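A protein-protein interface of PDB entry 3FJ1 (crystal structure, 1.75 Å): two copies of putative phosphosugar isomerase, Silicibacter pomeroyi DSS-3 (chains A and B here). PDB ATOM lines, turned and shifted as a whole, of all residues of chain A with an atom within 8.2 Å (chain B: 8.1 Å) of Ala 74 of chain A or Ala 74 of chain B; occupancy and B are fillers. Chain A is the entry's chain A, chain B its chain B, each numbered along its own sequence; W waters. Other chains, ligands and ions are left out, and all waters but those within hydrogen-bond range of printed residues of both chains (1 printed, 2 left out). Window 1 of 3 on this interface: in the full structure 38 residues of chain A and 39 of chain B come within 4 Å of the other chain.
OE2 of Glu 66 of chain B sits at hydrogen-bond distance from N of Val 73 of chain B (3.1 Å). The backbone NH of Thr 48 of chain A sits at hydrogen-bond distance from the backbone carbonyl oxygen of Ala 74 of chain A (2.9 Å). N of Thr 48 of chain B lies within hydrogen-bond range of O of Ala 74 of chain B. The backbone NH (N) of Val 73 of chain A is in hydrogen-bond range of the side-chain carboxylate (OE2) of Glu 66 of chain A (3.1 Å). The backbone NH (N) of Ala 74 of chain A lies within hydrogen-bond range of the backbone carbonyl oxygen (O) of Val 46 of chain A (2.8 Å). The backbone NH (N) of Val 46 of chain A sits at hydrogen-bond distance from the backbone carbonyl oxygen (O) of Pro 72 of chain A (3.0 Å).
Phe 45 of chain A touches Pro 72 of chain B (CE2 to CG, 3.6 Å). Leu 76 of chain B touches Glu 66 of chain A (CD2 to OE2, 3.97 Å). CG of Pro 72 of chain A touches CZ of Phe 45 of chain B (3.5 Å). Pro 72 of chain A touches Leu 90 of chain B (CB to CD2, 3.9 Å). Ala 74 of chain B touches Val 73 of chain A. Val 73 of chain B touches Ala 74 of chain A (O to CB, 3.3 Å). Ala 74 of chain A touches Ala 74 of chain B. Glu 66 of chain B touches Leu 76 of chain A. CD2 of Leu 88 of chain A touches O of Glu 66 of chain B, at 3.7 Å.
Ala 47 of chain A touches none of the printed residues of chain B. Printed residues of chain B within 4 Å of Glu 66 of chain A: Leu 76. Ala 74 of chain A touches just these residues of chain B: Val 73 (3.3 Å) and Ala 74 (3.8 Å). Printed residues of chain A within 4 Å of Glu 66 of chain B: Leu 76 (3.9 Å) and Leu 88 (3.7 Å). Ala 74 of chain B touches just these residues of chain A: Val 73 and Ala 74. Printed residues of chain A within 4 Å of Leu 90 of chain B: Pro 72. The nearest residue of chain B that does not touch Ala 74 of chain A is Pro 72 of chain B (4.5 Å). The nearest printed residue of chain A that does not touch Ala 74 of chain B is Pro 72 of chain A (4.7 Å). The nearest printed residue of chain B that does not touch Glu 66 of chain A is Gly 77 of chain B (5.0 Å).
Of the 20 printed residues of chain B, 7 touch a printed residue of chain A. Hydrophobic or aromatic side chains of chain B that line the printed part of chain A: Phe 45, Pro 72, Ala 74, Leu 76 and Leu 90. Hydrophobic or aromatic side chains of chain A that line the printed part of chain B: Phe 45, Pro 72, Ala 74, Leu 76 and Leu 88. Among the printed residues, no Asp or Glu carboxylate lies within 4 Å of a Lys or Arg side-chain nitrogen of the other chain.
Glu 66 of chain A touches Leu 76 of chain B, and with the chains exchanged Leu 76 of chain A touches Glu 66 of chain B. Pro 72 of chain A touches Leu 90 of chain B, but with the chains exchanged Leu 90 of chain A does not touch Pro 72 of chain B (4.04 Å). Val 73 of chain A touches Ala 74 of chain B, and with the chains exchanged Ala 74 of chain A touches Val 73 of chain B. Ala 74 of chain B touches its own counterpart, Ala 74 of chain A. 20 positions are printed for both chains. Of the 9 pairs that touch across the chains among the printed residues, 7 have their exchanged pair printed and touching as well.
Water W1 lies within hydrogen-bond range of the backbone NH (N) of Ser 75 of chain B (2.9 Å) and the backbone NH (N) of Ser 75 of chain A (2.9 Å).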
ATOM      1  N   PHE A  45     -25.974   3.519   3.954  1.00  0.00           N
ATOM      2  CA  PHE A  45     -25.331   3.124   2.705  1.00  0.00           C
ATOM      3  C   PHE A  45     -26.310   3.249   1.553  1.00  0.00           C
ATOM      4  O   PHE A  45     -27.508   3.517   1.729  1.00  0.00           O
ATOM      5  CB  PHE A  45     -24.637   1.744   2.737  1.00  0.00           C
ATOM      6  CG  PHE A  45     -25.575   0.579   2.746  1.00  0.00           C
ATOM      7  CD1 PHE A  45     -26.143   0.144   3.923  1.00  0.00           C
ATOM      8  CD2 PHE A  45     -25.866  -0.099   1.573  1.00  0.00           C
ATOM      9  CE1 PHE A  45     -27.013  -0.963   3.942  1.00  0.00           C
ATOM     10  CE2 PHE A  45     -26.719  -1.194   1.579  1.00  0.00           C
ATOM     11  CZ  PHE A  45     -27.296  -1.625   2.766  1.00  0.00           C
ATOM     12  N   VAL A  46     -25.719   3.195   0.364  1.00  0.00           N
ATOM     13  CA  VAL A  46     -26.452   3.417  -0.877  1.00  0.00           C
ATOM     14  C   VAL A  46     -26.273   2.231  -1.824  1.00  0.00           C
ATOM     15  O   VAL A  46     -25.167   1.701  -1.945  1.00  0.00           O
ATOM     16  CB  VAL A  46     -25.965   4.689  -1.594  1.00  0.00           C
ATOM     17  CG1 VAL A  46     -26.795   4.937  -2.858  1.00  0.00           C
ATOM     18  CG2 VAL A  46     -26.020   5.917  -0.647  1.00  0.00           C
ATOM     19  N   ALA A  47     -27.342   1.849  -2.523  1.00  0.00           N
ATOM     20  CA  ALA A  47     -27.272   0.841  -3.574  1.00  0.00           C
ATOM     21  C   ALA A  47     -27.748   1.498  -4.854  1.00  0.00           C
ATOM     22  O   ALA A  47     -28.648   2.326  -4.806  1.00  0.00           O
ATOM     23  CB  ALA A  47     -28.133  -0.375  -3.264  1.00  0.00           C
ATOM     24  N   THR A  48     -27.106   1.214  -5.979  1.00  0.00           N
ATOM     25  CA  THR A  48     -27.552   1.762  -7.255  1.00  0.00           C
ATOM     26  C   THR A  48     -28.040   0.617  -8.153  1.00  0.00           C
ATOM     27  O   THR A  48     -27.561  -0.519  -8.063  1.00  0.00           O
ATOM     28  CB  THR A  48     -26.496   2.600  -8.004  1.00  0.00           C
ATOM     29  OG1 THR A  48     -25.361   1.773  -8.300  1.00  0.00           O
ATOM     30  CG2 THR A  48     -26.065   3.871  -7.175  1.00  0.00           C
ATOM     31  N   VAL A  49     -29.011   0.948  -8.998  1.00  0.00           N
ATOM     32  CA  VAL A  49     -29.637   0.024  -9.935  1.00  0.00           C
ATOM     33  C   VAL A  49     -29.763   0.746 -11.294  1.00  0.00           C
ATOM     34  O   VAL A  49     -30.470   1.754 -11.421  1.00  0.00           O
ATOM     35  CB  VAL A  49     -31.045  -0.448  -9.489  1.00  0.00           C
ATOM     36  CG1 VAL A  49     -31.628  -1.478 -10.475  1.00  0.00           C
ATOM     37  CG2 VAL A  49     -30.977  -1.017  -8.064  1.00  0.00           C
ATOM     38  N   ASP A  55     -25.929   3.574 -15.969  1.00  0.00           N
ATOM     39  CA  ASP A  55     -24.961   3.064 -14.994  1.00  0.00           C
ATOM     40  C   ASP A  55     -23.704   3.952 -14.871  1.00  0.00           C
ATOM     41  O   ASP A  55     -23.075   3.977 -13.837  1.00  0.00           O
ATOM     42  CB  ASP A  55     -24.604   1.614 -15.294  1.00  0.00           C
ATOM     43  CG  ASP A  55     -24.258   0.824 -14.046  1.00  0.00           C
ATOM     44  OD1 ASP A  55     -24.532   1.271 -12.907  1.00  0.00           O
ATOM     45  OD2 ASP A  55     -23.719  -0.278 -14.225  1.00  0.00           O
ATOM     46  N   CYS A  58     -24.675   6.417 -12.509  1.00  0.00           N
ATOM     47  CA  CYS A  58     -24.530   5.826 -11.172  1.00  0.00           C
ATOM     48  C   CYS A  58     -23.066   5.828 -10.676  1.00  0.00           C
ATOM     49  O   CYS A  58     -22.791   6.125  -9.515  1.00  0.00           O
ATOM     50  CB  CYS A  58     -25.137   4.453 -11.146  1.00  0.00           C
ATOM     51  SG  CYS A  58     -26.963   4.490 -11.094  1.00  0.00           S
ATOM     52  N   SER A  62     -21.891   7.666  -7.401  1.00  0.00           N
ATOM     53  CA  SER A  62     -21.233   6.892  -6.357  1.00  0.00           C
ATOM     54  C   SER A  62     -20.032   7.675  -5.834  1.00  0.00           C
ATOM     55  O   SER A  62     -19.863   7.822  -4.625  1.00  0.00           O
ATOM     56  CB  SER A  62     -20.822   5.511  -6.860  1.00  0.00           C
ATOM     57  OG  SER A  62     -21.963   4.813  -7.296  1.00  0.00           O
ATOM     58  N   GLU A  66     -19.901   9.263  -1.957  1.00  0.00           N
ATOM     59  CA  GLU A  66     -18.759   8.885  -1.143  1.00  0.00           C
ATOM     60  C   GLU A  66     -17.955  10.118  -0.758  1.00  0.00           C
ATOM     61  O   GLU A  66     -17.638  10.279   0.405  1.00  0.00           O
ATOM     62  CB  GLU A  66     -17.924   7.823  -1.865  1.00  0.00           C
ATOM     63  CG  GLU A  66     -18.639   6.461  -1.814  1.00  0.00           C
ATOM     64  CD  GLU A  66     -18.000   5.335  -2.640  1.00  0.00           C
ATOM     65  OE1 GLU A  66     -16.933   5.538  -3.274  1.00  0.00           O
ATOM     66  OE2 GLU A  66     -18.606   4.239  -2.655  1.00  0.00           O
ATOM     67  N   LEU A  71     -20.774   7.916   2.340  1.00  0.00           N
ATOM     68  CA  LEU A  71     -21.597   6.721   2.312  1.00  0.00           C
ATOM     69  C   LEU A  71     -21.089   5.774   1.252  1.00  0.00           C
ATOM     70  O   LEU A  71     -20.872   6.184   0.121  1.00  0.00           O
ATOM     71  CB  LEU A  71     -23.070   7.056   2.043  1.00  0.00           C
ATOM     72  CG  LEU A  71     -23.788   7.842   3.151  1.00  0.00           C
ATOM     73  CD1 LEU A  71     -25.224   8.131   2.747  1.00  0.00           C
ATOM     74  CD2 LEU A  71     -23.752   7.093   4.489  1.00  0.00           C
ATOM     75  N   PRO A  72     -20.860   4.511   1.629  1.00  0.00           N
ATOM     76  CA  PRO A  72     -20.423   3.521   0.646  1.00  0.00           C
ATOM     77  C   PRO A  72     -21.594   3.210  -0.313  1.00  0.00           C
ATOM     78  O   PRO A  72     -22.772   3.192   0.096  1.00  0.00           O
ATOM     79  CB  PRO A  72     -20.027   2.333   1.513  1.00  0.00           C
ATOM     80  CG  PRO A  72     -20.835   2.482   2.742  1.00  0.00           C
ATOM     81  CD  PRO A  72     -21.027   3.933   2.970  1.00  0.00           C
ATOM     82  N   VAL A  73     -21.269   2.979  -1.575  1.00  0.00           N
ATOM     83  CA  VAL A  73     -22.266   2.782  -2.636  1.00  0.00           C
ATOM     84  C   VAL A  73     -22.019   1.451  -3.343  1.00  0.00           C
ATOM     85  O   VAL A  73     -20.954   1.224  -3.943  1.00  0.00           O
ATOM     86  CB  VAL A  73     -22.194   3.918  -3.661  1.00  0.00           C
ATOM     87  CG1 VAL A  73     -23.318   3.800  -4.713  1.00  0.00           C
ATOM     88  CG2 VAL A  73     -22.259   5.301  -2.945  1.00  0.00           C
ATOM     89  N   ALA A  74     -22.986   0.568  -3.235  1.00  0.00           N
ATOM     90  CA  ALA A  74     -22.916  -0.722  -3.876  1.00  0.00           C
ATOM     91  C   ALA A  74     -23.727  -0.735  -5.163  1.00  0.00           C
ATOM     92  O   ALA A  74     -24.928  -0.440  -5.134  1.00  0.00           O
ATOM     93  CB  ALA A  74     -23.468  -1.805  -2.935  1.00  0.00           C
ATOM     94  N   SER A  75     -23.098  -1.105  -6.280  1.00  0.00           N
ATOM     95  CA  SER A  75     -23.825  -1.302  -7.542  1.00  0.00           C
ATOM     96  C   SER A  75     -24.397  -2.725  -7.593  1.00  0.00           C
ATOM     97  O   SER A  75     -23.648  -3.716  -7.591  1.00  0.00           O
ATOM     98  CB  SER A  75     -22.894  -1.087  -8.745  1.00  0.00           C
ATOM     99  OG  SER A  75     -23.486  -1.490  -9.954  1.00  0.00           O
ATOM    100  N   LEU A  76     -25.721  -2.818  -7.602  1.00  0.00           N
ATOM    101  CA  LEU A  76     -26.408  -4.078  -7.600  1.00  0.00           C
ATOM    102  C   LEU A  76     -26.704  -4.627  -8.987  1.00  0.00           C
ATOM    103  O   LEU A  76     -27.428  -4.007  -9.769  1.00  0.00           O
ATOM    104  CB  LEU A  76     -27.734  -3.951  -6.825  1.00  0.00           C
ATOM    105  CG  LEU A  76     -27.721  -3.627  -5.322  1.00  0.00           C
ATOM    106  CD1 LEU A  76     -29.185  -3.538  -4.775  1.00  0.00           C
ATOM    107  CD2 LEU A  76     -26.852  -4.612  -4.541  1.00  0.00           C
ATOM    108  N   GLY A  77     -26.175  -5.814  -9.278  1.00  0.00           N
ATOM    109  CA  GLY A  77     -26.432  -6.454 -10.553  1.00  0.00           C
ATOM    110  C   GLY A  77     -27.894  -6.865 -10.595  1.00  0.00           C
ATOM    111  O   GLY A  77     -28.314  -7.635  -9.733  1.00  0.00           O
ATOM    112  N   LEU A  88     -31.878  -9.717   0.045  1.00  0.00           N
ATOM    113  CA  LEU A  88     -30.764  -8.894   0.504  1.00  0.00           C
ATOM    114  C   LEU A  88     -31.119  -8.169   1.804  1.00  0.00           C
ATOM    115  O   LEU A  88     -32.295  -8.004   2.143  1.00  0.00           O
ATOM    116  CB  LEU A  88     -30.358  -7.873  -0.580  1.00  0.00           C
ATOM    117  CG  LEU A  88     -29.860  -8.464  -1.919  1.00  0.00           C
ATOM    118  CD1 LEU A  88     -29.388  -7.374  -2.829  1.00  0.00           C
ATOM    119  CD2 LEU A  88     -28.738  -9.446  -1.674  1.00  0.00           C
ATOM    120  N   LEU A  90     -31.155  -4.878   3.156  1.00  0.00           N
ATOM    121  CA  LEU A  90     -31.112  -3.491   2.700  1.00  0.00           C
ATOM    122  C   LEU A  90     -31.805  -2.466   3.623  1.00  0.00           C
ATOM    123  O   LEU A  90     -32.062  -1.326   3.212  1.00  0.00           O
ATOM    124  CB  LEU A  90     -31.647  -3.393   1.268  1.00  0.00           C
ATOM    125  CG  LEU A  90     -30.816  -4.127   0.208  1.00  0.00           C
ATOM    126  CD1 LEU A  90     -31.519  -4.104  -1.166  1.00  0.00           C
ATOM    127  CD2 LEU A  90     -29.454  -3.505   0.106  1.00  0.00           C
ATOM    128  N   LEU A  94     -30.384   3.530   1.084  1.00  0.00           N
ATOM    129  CA  LEU A  94     -31.034   4.275  -0.007  1.00  0.00           C
ATOM    130  C   LEU A  94     -30.783   3.402  -1.236  1.00  0.00           C
ATOM    131  O   LEU A  94     -29.628   3.010  -1.495  1.00  0.00           O
ATOM    132  CB  LEU A  94     -30.340   5.608  -0.273  1.00  0.00           C
ATOM    133  CG  LEU A  94     -30.613   6.352  -1.604  1.00  0.00           C
ATOM    134  CD1 LEU A  94     -32.109   6.693  -1.786  1.00  0.00           C
ATOM    135  CD2 LEU A  94     -29.830   7.667  -1.739  1.00  0.00           C
ATOM    136  N   CYS A  95     -31.815   3.083  -1.995  1.00  0.00           N
ATOM    137  CA  CYS A  95     -31.613   2.450  -3.295  1.00  0.00           C
ATOM    138  C   CYS A  95     -31.927   3.483  -4.390  1.00  0.00           C
ATOM    139  O   CYS A  95     -33.060   3.952  -4.505  1.00  0.00           O
ATOM    140  CB  CYS A  95     -32.469   1.214  -3.471  1.00  0.00           C
ATOM    141  SG  CYS A  95     -32.253   0.458  -5.119  1.00  0.00           S
ATOM    142  N   LEU A  96     -30.919   3.826  -5.195  1.00  0.00           N
ATOM    143  CA  LEU A  96     -31.074   4.811  -6.229  1.00  0.00           C
ATOM    144  C   LEU A  96     -31.148   4.104  -7.592  1.00  0.00           C
ATOM    145  O   LEU A  96     -30.173   3.482  -7.995  1.00  0.00           O
ATOM    146  CB  LEU A  96     -29.897   5.768  -6.162  1.00  0.00           C
ATOM    147  CG  LEU A  96     -29.997   6.999  -7.006  1.00  0.00           C
ATOM    148  CD1 LEU A  96     -31.176   7.897  -6.588  1.00  0.00           C
ATOM    149  CD2 LEU A  96     -28.664   7.736  -6.901  1.00  0.00           C
ATOM    150  N   PHE B  45     -22.685  -5.008   5.552  1.00  0.00           N
ATOM    151  CA  PHE B  45     -22.297  -4.969   4.141  1.00  0.00           C
ATOM    152  C   PHE B  45     -20.808  -5.290   3.982  1.00  0.00           C
ATOM    153  O   PHE B  45     -20.046  -5.408   4.965  1.00  0.00           O
ATOM    154  CB  PHE B  45     -22.676  -3.652   3.458  1.00  0.00           C
ATOM    155  CG  PHE B  45     -21.873  -2.495   3.916  1.00  0.00           C
ATOM    156  CD1 PHE B  45     -22.238  -1.806   5.052  1.00  0.00           C
ATOM    157  CD2 PHE B  45     -20.735  -2.118   3.225  1.00  0.00           C
ATOM    158  CE1 PHE B  45     -21.461  -0.707   5.500  1.00  0.00           C
ATOM    159  CE2 PHE B  45     -19.961  -1.059   3.654  1.00  0.00           C
ATOM    160  CZ  PHE B  45     -20.331  -0.350   4.796  1.00  0.00           C
ATOM    161  N   VAL B  46     -20.433  -5.496   2.728  1.00  0.00           N
ATOM    162  CA  VAL B  46     -19.091  -5.855   2.378  1.00  0.00           C
ATOM    163  C   VAL B  46     -18.593  -4.817   1.358  1.00  0.00           C
ATOM    164  O   VAL B  46     -19.365  -4.368   0.517  1.00  0.00           O
ATOM    165  CB  VAL B  46     -19.063  -7.236   1.694  1.00  0.00           C
ATOM    166  CG1 VAL B  46     -17.653  -7.584   1.266  1.00  0.00           C
ATOM    167  CG2 VAL B  46     -19.662  -8.368   2.634  1.00  0.00           C
ATOM    168  N   ALA B  47     -17.312  -4.457   1.426  1.00  0.00           N
ATOM    169  CA  ALA B  47     -16.680  -3.588   0.453  1.00  0.00           C
ATOM    170  C   ALA B  47     -15.536  -4.404  -0.131  1.00  0.00           C
ATOM    171  O   ALA B  47     -14.952  -5.260   0.569  1.00  0.00           O
ATOM    172  CB  ALA B  47     -16.129  -2.333   1.079  1.00  0.00           C
ATOM    173  N   THR B  48     -15.238  -4.174  -1.400  1.00  0.00           N
ATOM    174  CA  THR B  48     -14.124  -4.866  -2.048  1.00  0.00           C
ATOM    175  C   THR B  48     -13.136  -3.830  -2.594  1.00  0.00           C
ATOM    176  O   THR B  48     -13.514  -2.716  -3.009  1.00  0.00           O
ATOM    177  CB  THR B  48     -14.580  -5.830  -3.185  1.00  0.00           C
ATOM    178  OG1 THR B  48     -15.161  -5.066  -4.256  1.00  0.00           O
ATOM    179  CG2 THR B  48     -15.593  -6.908  -2.648  1.00  0.00           C
ATOM    180  N   VAL B  49     -11.871  -4.219  -2.598  1.00  0.00           N
ATOM    181  CA  VAL B  49     -10.789  -3.393  -3.051  1.00  0.00           C
ATOM    182  C   VAL B  49      -9.863  -4.255  -3.919  1.00  0.00           C
ATOM    183  O   VAL B  49      -9.210  -5.159  -3.401  1.00  0.00           O
ATOM    184  CB  VAL B  49     -10.014  -2.770  -1.889  1.00  0.00           C
ATOM    185  CG1 VAL B  49      -8.870  -1.909  -2.425  1.00  0.00           C
ATOM    186  CG2 VAL B  49     -10.991  -1.948  -0.982  1.00  0.00           C
ATOM    187  N   ASP B  55      -9.988  -7.792  -9.558  1.00  0.00           N
ATOM    188  CA  ASP B  55     -11.329  -7.179  -9.498  1.00  0.00           C
ATOM    189  C   ASP B  55     -12.398  -8.093 -10.095  1.00  0.00           C
ATOM    190  O   ASP B  55     -13.538  -8.070  -9.669  1.00  0.00           O
ATOM    191  CB  ASP B  55     -11.337  -5.756 -10.067  1.00  0.00           C
ATOM    192  CG  ASP B  55     -12.418  -4.861  -9.447  1.00  0.00           C
ATOM    193  OD1 ASP B  55     -13.009  -5.191  -8.407  1.00  0.00           O
ATOM    194  OD2 ASP B  55     -12.683  -3.807 -10.060  1.00  0.00           O
ATOM    195  N   CYS B  58     -13.155 -10.257  -7.287  1.00  0.00           N
ATOM    196  CA  CYS B  58     -14.144  -9.517  -6.473  1.00  0.00           C
ATOM    197  C   CYS B  58     -15.592  -9.564  -7.020  1.00  0.00           C
ATOM    198  O   CYS B  58     -16.537  -9.741  -6.255  1.00  0.00           O
ATOM    199  CB  CYS B  58     -13.693  -8.105  -6.183  1.00  0.00           C
ATOM    200  SG  CYS B  58     -12.295  -8.102  -5.035  1.00  0.00           S
ATOM    201  N   SER B  62     -18.637 -11.045  -5.014  1.00  0.00           N
ATOM    202  CA  SER B  62     -19.760 -10.149  -4.765  1.00  0.00           C
ATOM    203  C   SER B  62     -21.071 -10.899  -4.977  1.00  0.00           C
ATOM    204  O   SER B  62     -21.943 -10.907  -4.108  1.00  0.00           O
ATOM    205  CB  SER B  62     -19.720  -8.932  -5.688  1.00  0.00           C
ATOM    206  OG  SER B  62     -20.815  -8.073  -5.399  1.00  0.00           O
ATOM    207  N   GLU B  66     -23.732 -12.041  -1.992  1.00  0.00           N
ATOM    208  CA  GLU B  66     -25.123 -11.628  -2.074  1.00  0.00           C
ATOM    209  C   GLU B  66     -26.095 -12.803  -2.102  1.00  0.00           C
ATOM    210  O   GLU B  66     -27.128 -12.770  -1.426  1.00  0.00           O
ATOM    211  CB  GLU B  66     -25.351 -10.664  -3.245  1.00  0.00           C
ATOM    212  CG  GLU B  66     -24.657  -9.327  -2.992  1.00  0.00           C
ATOM    213  CD  GLU B  66     -24.623  -8.375  -4.147  1.00  0.00           C
ATOM    214  OE1 GLU B  66     -25.063  -8.720  -5.261  1.00  0.00           O
ATOM    215  OE2 GLU B  66     -24.109  -7.255  -3.914  1.00  0.00           O
ATOM    216  N   LEU B  71     -25.770 -10.107   1.763  1.00  0.00           N
ATOM    217  CA  LEU B  71     -25.110  -8.857   2.095  1.00  0.00           C
ATOM    218  C   LEU B  71     -24.790  -8.084   0.837  1.00  0.00           C
ATOM    219  O   LEU B  71     -24.185  -8.633  -0.092  1.00  0.00           O
ATOM    220  CB  LEU B  71     -23.811  -9.105   2.870  1.00  0.00           C
ATOM    221  CG  LEU B  71     -23.984  -9.834   4.185  1.00  0.00           C
ATOM    222  CD1 LEU B  71     -22.597 -10.028   4.817  1.00  0.00           C
ATOM    223  CD2 LEU B  71     -24.929  -8.978   5.090  1.00  0.00           C
ATOM    224  N   PRO B  72     -25.169  -6.803   0.797  1.00  0.00           N
ATOM    225  CA  PRO B  72     -24.777  -6.029  -0.375  1.00  0.00           C
ATOM    226  C   PRO B  72     -23.271  -5.762  -0.392  1.00  0.00           C
ATOM    227  O   PRO B  72     -22.645  -5.579   0.649  1.00  0.00           O
ATOM    228  CB  PRO B  72     -25.569  -4.728  -0.208  1.00  0.00           C
ATOM    229  CG  PRO B  72     -25.734  -4.595   1.249  1.00  0.00           C
ATOM    230  CD  PRO B  72     -25.936  -5.979   1.750  1.00  0.00           C
ATOM    231  N   VAL B  73     -22.712  -5.763  -1.582  1.00  0.00           N
ATOM    232  CA  VAL B  73     -21.265  -5.630  -1.777  1.00  0.00           C
ATOM    233  C   VAL B  73     -20.918  -4.390  -2.607  1.00  0.00           C
ATOM    234  O   VAL B  73     -21.367  -4.237  -3.748  1.00  0.00           O
ATOM    235  CB  VAL B  73     -20.704  -6.893  -2.438  1.00  0.00           C
ATOM    236  CG1 VAL B  73     -19.171  -6.742  -2.609  1.00  0.00           C
ATOM    237  CG2 VAL B  73     -21.051  -8.157  -1.597  1.00  0.00           C
ATOM    238  N   ALA B  74     -20.107  -3.517  -2.022  1.00  0.00           N
ATOM    239  CA  ALA B  74     -19.717  -2.286  -2.667  1.00  0.00           C
ATOM    240  C   ALA B  74     -18.282  -2.343  -3.178  1.00  0.00           C
ATOM    241  O   ALA B  74     -17.372  -2.630  -2.422  1.00  0.00           O
ATOM    242  CB  ALA B  74     -19.877  -1.132  -1.687  1.00  0.00           C
ATOM    243  N   SER B  75     -18.087  -2.121  -4.468  1.00  0.00           N
ATOM    244  CA  SER B  75     -16.734  -2.041  -5.028  1.00  0.00           C
ATOM    245  C   SER B  75     -16.223  -0.598  -4.828  1.00  0.00           C
ATOM    246  O   SER B  75     -16.805   0.342  -5.361  1.00  0.00           O
ATOM    247  CB  SER B  75     -16.763  -2.386  -6.494  1.00  0.00           C
ATOM    248  OG  SER B  75     -15.482  -2.238  -7.083  1.00  0.00           O
ATOM    249  N   LEU B  76     -15.152  -0.439  -4.048  1.00  0.00           N
ATOM    250  CA  LEU B  76     -14.571   0.871  -3.732  1.00  0.00           C
ATOM    251  C   LEU B  76     -13.449   1.297  -4.681  1.00  0.00           C
ATOM    252  O   LEU B  76     -12.385   0.635  -4.769  1.00  0.00           O
ATOM    253  CB  LEU B  76     -14.002   0.861  -2.307  1.00  0.00           C
ATOM    254  CG  LEU B  76     -14.909   0.618  -1.089  1.00  0.00           C
ATOM    255  CD1 LEU B  76     -14.119   0.790   0.220  1.00  0.00           C
ATOM    256  CD2 LEU B  76     -16.084   1.561  -1.158  1.00  0.00           C
ATOM    257  N   GLY B  77     -13.665   2.429  -5.349  1.00  0.00           N
ATOM    258  CA  GLY B  77     -12.687   2.974  -6.268  1.00  0.00           C
ATOM    259  C   GLY B  77     -11.497   3.383  -5.453  1.00  0.00           C
ATOM    260  O   GLY B  77     -11.628   4.249  -4.595  1.00  0.00           O
ATOM    261  N   LEU B  90     -17.699   3.141   7.268  1.00  0.00           N
ATOM    262  CA  LEU B  90     -17.612   1.666   7.092  1.00  0.00           C
ATOM    263  C   LEU B  90     -17.742   0.892   8.407  1.00  0.00           C
ATOM    264  O   LEU B  90     -17.294  -0.255   8.512  1.00  0.00           O
ATOM    265  CB  LEU B  90     -16.311   1.291   6.391  1.00  0.00           C
ATOM    266  CG  LEU B  90     -16.077   1.984   5.041  1.00  0.00           C
ATOM    267  CD1 LEU B  90     -14.678   1.667   4.486  1.00  0.00           C
ATOM    268  CD2 LEU B  90     -17.151   1.563   4.061  1.00  0.00           C
ATOM    269  N   LEU B  94     -17.219  -5.521   6.369  1.00  0.00           N
ATOM    270  CA  LEU B  94     -16.101  -6.384   5.991  1.00  0.00           C
ATOM    271  C   LEU B  94     -15.467  -5.644   4.793  1.00  0.00           C
ATOM    272  O   LEU B  94     -16.161  -5.216   3.897  1.00  0.00           O
ATOM    273  CB  LEU B  94     -16.543  -7.777   5.513  1.00  0.00           C
ATOM    274  CG  LEU B  94     -15.503  -8.594   4.734  1.00  0.00           C
ATOM    275  CD1 LEU B  94     -14.233  -8.900   5.536  1.00  0.00           C
ATOM    276  CD2 LEU B  94     -16.131  -9.915   4.220  1.00  0.00           C
ATOM    277  N   CYS B  95     -14.160  -5.479   4.781  1.00  0.00           N
ATOM    278  CA  CYS B  95     -13.511  -4.947   3.578  1.00  0.00           C
ATOM    279  C   CYS B  95     -12.597  -6.061   3.068  1.00  0.00           C
ATOM    280  O   CYS B  95     -11.667  -6.497   3.740  1.00  0.00           O
ATOM    281  CB  CYS B  95     -12.771  -3.652   3.807  1.00  0.00           C
ATOM    282  SG  CYS B  95     -11.785  -3.140   2.326  1.00  0.00           S
ATOM    283  N   LEU B  96     -12.894  -6.562   1.873  1.00  0.00           N
ATOM    284  CA  LEU B  96     -12.117  -7.622   1.296  1.00  0.00           C
ATOM    285  C   LEU B  96     -11.218  -7.043   0.214  1.00  0.00           C
ATOM    286  O   LEU B  96     -11.720  -6.517  -0.762  1.00  0.00           O
ATOM    287  CB  LEU B  96     -13.057  -8.665   0.711  1.00  0.00           C
ATOM    288  CG  LEU B  96     -12.448  -9.952   0.211  1.00  0.00           C
ATOM    289  CD1 LEU B  96     -11.673 -10.698   1.341  1.00  0.00           C
ATOM    290  CD2 LEU B  96     -13.584 -10.829  -0.372  1.00  0.00           C
HETATM  291  O   HOH W   1     -20.249  -1.743  -6.389  1.00  0.00           O
